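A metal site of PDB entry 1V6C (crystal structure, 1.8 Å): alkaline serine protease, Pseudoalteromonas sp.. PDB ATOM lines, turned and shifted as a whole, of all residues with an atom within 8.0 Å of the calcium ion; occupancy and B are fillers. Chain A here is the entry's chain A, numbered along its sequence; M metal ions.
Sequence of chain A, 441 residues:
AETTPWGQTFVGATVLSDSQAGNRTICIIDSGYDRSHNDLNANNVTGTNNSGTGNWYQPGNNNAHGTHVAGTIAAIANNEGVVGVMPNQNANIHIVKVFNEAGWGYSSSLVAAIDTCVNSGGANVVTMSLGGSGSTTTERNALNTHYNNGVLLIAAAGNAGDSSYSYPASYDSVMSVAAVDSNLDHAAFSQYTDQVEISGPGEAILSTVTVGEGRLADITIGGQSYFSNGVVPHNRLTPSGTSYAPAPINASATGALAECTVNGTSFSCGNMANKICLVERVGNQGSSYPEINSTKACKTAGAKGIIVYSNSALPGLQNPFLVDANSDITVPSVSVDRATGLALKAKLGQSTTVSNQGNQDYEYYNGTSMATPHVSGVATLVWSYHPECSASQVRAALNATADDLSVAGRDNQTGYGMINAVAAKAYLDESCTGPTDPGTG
The calcium ion is bound by the backbone carbonyl oxygen (O) of Glu 80 (2.2 Å), the backbone carbonyl oxygen (O) of Ile 76 (2.3 Å), the side-chain carboxylate (OE1) of Glu 2 (2.4 Å), the backbone carbonyl oxygen (O) of Val 82 (2.4 Å), the side-chain carboxylate (OD1) of Asp 39 (2.4 Å), the side-chain amide oxygen (OD1) of Asn 78 (2.4 Å) and the side-chain carboxylate (OD2) of Asp 39 (2.5 Å).
The side-chain amide nitrogen of Asn 38 sits at hydrogen-bond distance from the side-chain carboxylate of Glu 80, at 3.1 Å. N of Asn 79 lies close to OE1 of Glu 2 (3.4 Å).
The nearest printed residue that does not touch the calcium ion is Gly 81 (4.1 Å).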
ATOM      1  N   ALA A   1     -16.513   8.668   1.080  1.00  0.00           N
ATOM      2  CA  ALA A   1     -17.562   8.344   0.075  1.00  0.00           C
ATOM      3  C   ALA A   1     -18.922   8.284   0.761  1.00  0.00           C
ATOM      4  O   ALA A   1     -19.053   7.736   1.851  1.00  0.00           O
ATOM      5  CB  ALA A   1     -17.250   7.003  -0.590  1.00  0.00           C
ATOM      6  N   GLU A   2     -19.928   8.844   0.108  1.00  0.00           N
ATOM      7  CA  GLU A   2     -21.276   8.862   0.651  1.00  0.00           C
ATOM      8  C   GLU A   2     -22.238   8.144  -0.283  1.00  0.00           C
ATOM      9  O   GLU A   2     -22.258   8.393  -1.486  1.00  0.00           O
ATOM     10  CB  GLU A   2     -21.718  10.309   0.853  1.00  0.00           C
ATOM     11  CG  GLU A   2     -23.104  10.497   1.429  1.00  0.00           C
ATOM     12  CD  GLU A   2     -23.349  11.925   1.832  1.00  0.00           C
ATOM     13  OE1 GLU A   2     -23.341  12.220   3.049  1.00  0.00           O
ATOM     14  OE2 GLU A   2     -23.519  12.769   0.924  1.00  0.00           O
ATOM     15  N   THR A   3     -23.047   7.250   0.288  1.00  0.00           N
ATOM     16  CA  THR A   3     -23.997   6.485  -0.507  1.00  0.00           C
ATOM     17  C   THR A   3     -25.426   6.953  -0.320  1.00  0.00           C
ATOM     18  O   THR A   3     -25.819   7.427   0.753  1.00  0.00           O
ATOM     19  CB  THR A   3     -23.907   4.984  -0.141  1.00  0.00           C
ATOM     20  OG1 THR A   3     -22.591   4.505  -0.424  1.00  0.00           O
ATOM     21  CG2 THR A   3     -24.912   4.167  -0.930  1.00  0.00           C
ATOM     22  N   HIS A  37     -23.096  10.530  16.543  1.00  0.00           N
ATOM     23  CA  HIS A  37     -22.869  10.025  15.194  1.00  0.00           C
ATOM     24  C   HIS A  37     -22.521  11.142  14.218  1.00  0.00           C
ATOM     25  O   HIS A  37     -23.179  12.178  14.202  1.00  0.00           O
ATOM     26  CB  HIS A  37     -24.122   9.302  14.709  1.00  0.00           C
ATOM     27  CG  HIS A  37     -23.897   8.464  13.487  1.00  0.00           C
ATOM     28  ND1 HIS A  37     -24.042   7.091  13.494  1.00  0.00           N
ATOM     29  CD2 HIS A  37     -23.519   8.790  12.238  1.00  0.00           C
ATOM     30  CE1 HIS A  37     -23.754   6.608  12.294  1.00  0.00           C
ATOM     31  NE2 HIS A  37     -23.428   7.626  11.507  1.00  0.00           N
ATOM     32  N   ASN A  38     -21.496  10.929  13.398  1.00  0.00           N
ATOM     33  CA  ASN A  38     -21.079  11.948  12.426  1.00  0.00           C
ATOM     34  C   ASN A  38     -22.186  12.375  11.470  1.00  0.00           C
ATOM     35  O   ASN A  38     -22.238  13.538  11.061  1.00  0.00           O
ATOM     36  CB  ASN A  38     -19.879  11.453  11.599  1.00  0.00           C
ATOM     37  CG  ASN A  38     -18.609  11.338  12.415  1.00  0.00           C
ATOM     38  OD1 ASN A  38     -18.508  11.890  13.507  1.00  0.00           O
ATOM     39  ND2 ASN A  38     -17.624  10.627  11.873  1.00  0.00           N
ATOM     40  N   ASP A  39     -23.060  11.456  11.101  1.00  0.00           N
ATOM     41  CA  ASP A  39     -24.140  11.773  10.167  1.00  0.00           C
ATOM     42  C   ASP A  39     -25.398  12.334  10.844  1.00  0.00           C
ATOM     43  O   ASP A  39     -26.389  12.595  10.176  1.00  0.00           O
ATOM     44  CB  ASP A  39     -24.497  10.540   9.337  1.00  0.00           C
ATOM     45  CG  ASP A  39     -23.976  10.622   7.911  1.00  0.00           C
ATOM     46  OD1 ASP A  39     -23.087  11.457   7.637  1.00  0.00           O
ATOM     47  OD2 ASP A  39     -24.447   9.848   7.051  1.00  0.00           O
ATOM     48  N   LEU A  40     -25.333  12.553  12.152  1.00  0.00           N
ATOM     49  CA  LEU A  40     -26.488  13.079  12.894  1.00  0.00           C
ATOM     50  C   LEU A  40     -26.189  14.211  13.876  1.00  0.00           C
ATOM     51  O   LEU A  40     -27.083  14.981  14.239  1.00  0.00           O
ATOM     52  CB  LEU A  40     -27.169  11.941  13.660  1.00  0.00           C
ATOM     53  CG  LEU A  40     -27.807  10.817  12.846  1.00  0.00           C
ATOM     54  CD1 LEU A  40     -28.242   9.712  13.796  1.00  0.00           C
ATOM     55  CD2 LEU A  40     -28.996  11.355  12.048  1.00  0.00           C
ATOM     56  N   ALA A  74     -33.088  12.240   8.234  1.00  0.00           N
ATOM     57  CA  ALA A  74     -32.132  13.330   8.113  1.00  0.00           C
ATOM     58  C   ALA A  74     -30.638  13.038   8.183  1.00  0.00           C
ATOM     59  O   ALA A  74     -29.870  13.891   8.648  1.00  0.00           O
ATOM     60  CB  ALA A  74     -32.480  14.401   9.144  1.00  0.00           C
ATOM     61  N   ALA A  75     -30.189  11.864   7.735  1.00  0.00           N
ATOM     62  CA  ALA A  75     -28.749  11.597   7.749  1.00  0.00           C
ATOM     63  C   ALA A  75     -28.122  12.758   6.969  1.00  0.00           C
ATOM     64  O   ALA A  75     -28.576  13.092   5.870  1.00  0.00           O
ATOM     65  CB  ALA A  75     -28.449  10.270   7.068  1.00  0.00           C
ATOM     66  N   ILE A  76     -27.081  13.358   7.527  1.00  0.00           N
ATOM     67  CA  ILE A  76     -26.432  14.520   6.927  1.00  0.00           C
ATOM     68  C   ILE A  76     -25.593  14.306   5.653  1.00  0.00           C
ATOM     69  O   ILE A  76     -24.818  13.350   5.550  1.00  0.00           O
ATOM     70  CB  ILE A  76     -25.562  15.248   7.980  1.00  0.00           C
ATOM     71  CG1 ILE A  76     -26.447  15.665   9.153  1.00  0.00           C
ATOM     72  CG2 ILE A  76     -24.879  16.482   7.366  1.00  0.00           C
ATOM     73  CD1 ILE A  76     -25.678  16.170  10.375  1.00  0.00           C
ATOM     74  N   ALA A  77     -25.755  15.228   4.706  1.00  0.00           N
ATOM     75  CA  ALA A  77     -24.995  15.189   3.460  1.00  0.00           C
ATOM     76  C   ALA A  77     -23.601  15.708   3.798  1.00  0.00           C
ATOM     77  O   ALA A  77     -23.457  16.870   4.209  1.00  0.00           O
ATOM     78  CB  ALA A  77     -25.666  16.078   2.407  1.00  0.00           C
ATOM     79  N   ASN A  78     -22.587  14.866   3.637  1.00  0.00           N
ATOM     80  CA  ASN A  78     -21.220  15.263   3.971  1.00  0.00           C
ATOM     81  C   ASN A  78     -20.137  14.347   3.412  1.00  0.00           C
ATOM     82  O   ASN A  78     -19.074  14.198   4.019  1.00  0.00           O
ATOM     83  CB  ASN A  78     -21.080  15.330   5.485  1.00  0.00           C
ATOM     84  CG  ASN A  78     -21.555  14.046   6.162  1.00  0.00           C
ATOM     85  OD1 ASN A  78     -21.717  13.014   5.507  1.00  0.00           O
ATOM     86  ND2 ASN A  78     -21.755  14.108   7.472  1.00  0.00           N
ATOM     87  N   ASN A  79     -20.388  13.719   2.265  1.00  0.00           N
ATOM     88  CA  ASN A  79     -19.374  12.848   1.654  1.00  0.00           C
ATOM     89  C   ASN A  79     -18.954  11.633   2.504  1.00  0.00           C
ATOM     90  O   ASN A  79     -17.869  11.074   2.303  1.00  0.00           O
ATOM     91  CB  ASN A  79     -18.137  13.660   1.279  1.00  0.00           C
ATOM     92  CG  ASN A  79     -17.156  12.878   0.411  1.00  0.00           C
ATOM     93  OD1 ASN A  79     -17.507  12.418  -0.678  1.00  0.00           O
ATOM     94  ND2 ASN A  79     -15.926  12.728   0.886  1.00  0.00           N
ATOM     95  N   GLU A  80     -19.795  11.239   3.454  1.00  0.00           N
ATOM     96  CA  GLU A  80     -19.496  10.064   4.277  1.00  0.00           C
ATOM     97  C   GLU A  80     -20.823   9.449   4.713  1.00  0.00           C
ATOM     98  O   GLU A  80     -21.826  10.154   4.826  1.00  0.00           O
ATOM     99  CB  GLU A  80     -18.667  10.455   5.515  1.00  0.00           C
ATOM    100  CG  GLU A  80     -19.444  10.569   6.823  1.00  0.00           C
ATOM    101  CD  GLU A  80     -18.557  10.976   7.992  1.00  0.00           C
ATOM    102  OE1 GLU A  80     -18.064  12.124   7.998  1.00  0.00           O
ATOM    103  OE2 GLU A  80     -18.347  10.148   8.901  1.00  0.00           O
ATOM    104  N   GLY A  81     -20.827   8.142   4.932  1.00  0.00           N
ATOM    105  CA  GLY A  81     -22.057   7.478   5.343  1.00  0.00           C
ATOM    106  C   GLY A  81     -23.172   7.514   4.309  1.00  0.00           C
ATOM    107  O   GLY A  81     -22.979   7.108   3.169  1.00  0.00           O
ATOM    108  N   VAL A  82     -24.333   8.012   4.713  1.00  0.00           N
ATOM    109  CA  VAL A  82     -25.476   8.086   3.812  1.00  0.00           C
ATOM    110  C   VAL A  82     -26.134   9.459   3.866  1.00  0.00           C
ATOM    111  O   VAL A  82     -25.547  10.415   4.383  1.00  0.00           O
ATOM    112  CB  VAL A  82     -26.536   7.016   4.204  1.00  0.00           C
ATOM    113  CG1 VAL A  82     -25.923   5.621   4.159  1.00  0.00           C
ATOM    114  CG2 VAL A  82     -27.057   7.299   5.610  1.00  0.00           C
ATOM    115  N   VAL A  83     -27.331   9.555   3.306  1.00  0.00           N
ATOM    116  CA  VAL A  83     -28.097  10.785   3.288  1.00  0.00           C
ATOM    117  C   VAL A  83     -29.565  10.448   3.549  1.00  0.00           C
ATOM    118  O   VAL A  83     -30.060   9.405   3.099  1.00  0.00           O
ATOM    119  CB  VAL A  83     -27.982  11.534   1.925  1.00  0.00           C
ATOM    120  CG1 VAL A  83     -26.586  12.099   1.751  1.00  0.00           C
ATOM    121  CG2 VAL A  83     -28.311  10.586   0.786  1.00  0.00           C
ATOM    122  N   GLY A  84     -30.246  11.313   4.283  1.00  0.00           N
ATOM    123  CA  GLY A  84     -31.656  11.112   4.580  1.00  0.00           C
ATOM    124  C   GLY A  84     -32.522  11.961   3.666  1.00  0.00           C
ATOM    125  O   GLY A  84     -32.001  12.635   2.776  1.00  0.00           O
ATOM    126  N   PRO A  87     -31.235  16.005   4.202  1.00  0.00           N
ATOM    127  CA  PRO A  87     -29.842  15.927   4.630  1.00  0.00           C
ATOM    128  C   PRO A  87     -29.000  17.202   4.737  1.00  0.00           C
ATOM    129  O   PRO A  87     -27.830  17.117   5.114  1.00  0.00           O
ATOM    130  CB  PRO A  87     -29.254  14.982   3.601  1.00  0.00           C
ATOM    131  CG  PRO A  87     -29.882  15.520   2.331  1.00  0.00           C
ATOM    132  CD  PRO A  87     -31.341  15.789   2.752  1.00  0.00           C
ATOM    133  N   THR A 208     -28.165   5.025   9.472  1.00  0.00           N
ATOM    134  CA  THR A 208     -27.296   5.192  10.627  1.00  0.00           C
ATOM    135  C   THR A 208     -27.777   4.367  11.822  1.00  0.00           C
ATOM    136  O   THR A 208     -28.979   4.171  12.002  1.00  0.00           O
ATOM    137  CB  THR A 208     -27.291   6.660  11.076  1.00  0.00           C
ATOM    138  OG1 THR A 208     -28.645   7.112  11.245  1.00  0.00           O
ATOM    139  CG2 THR A 208     -26.583   7.547  10.054  1.00  0.00           C
ATOM    140  N   TYR A 362     -23.344   2.017  10.453  1.00  0.00           N
ATOM    141  CA  TYR A 362     -24.514   1.963   9.580  1.00  0.00           C
ATOM    142  C   TYR A 362     -24.929   0.495   9.490  1.00  0.00           C
ATOM    143  O   TYR A 362     -24.136  -0.394   9.779  1.00  0.00           O
ATOM    144  CB  TYR A 362     -24.166   2.474   8.176  1.00  0.00           C
ATOM    145  CG  TYR A 362     -23.571   3.865   8.176  1.00  0.00           C
ATOM    146  CD1 TYR A 362     -24.377   4.992   8.106  1.00  0.00           C
ATOM    147  CD2 TYR A 362     -22.194   4.046   8.337  1.00  0.00           C
ATOM    148  CE1 TYR A 362     -23.835   6.278   8.188  1.00  0.00           C
ATOM    149  CE2 TYR A 362     -21.640   5.317   8.435  1.00  0.00           C
ATOM    150  CZ  TYR A 362     -22.463   6.430   8.366  1.00  0.00           C
ATOM    151  OH  TYR A 362     -21.927   7.690   8.475  1.00  0.00           O
HETATM  152 CA    CA M   1     -23.567  11.452   5.277  1.00  0.00          CA
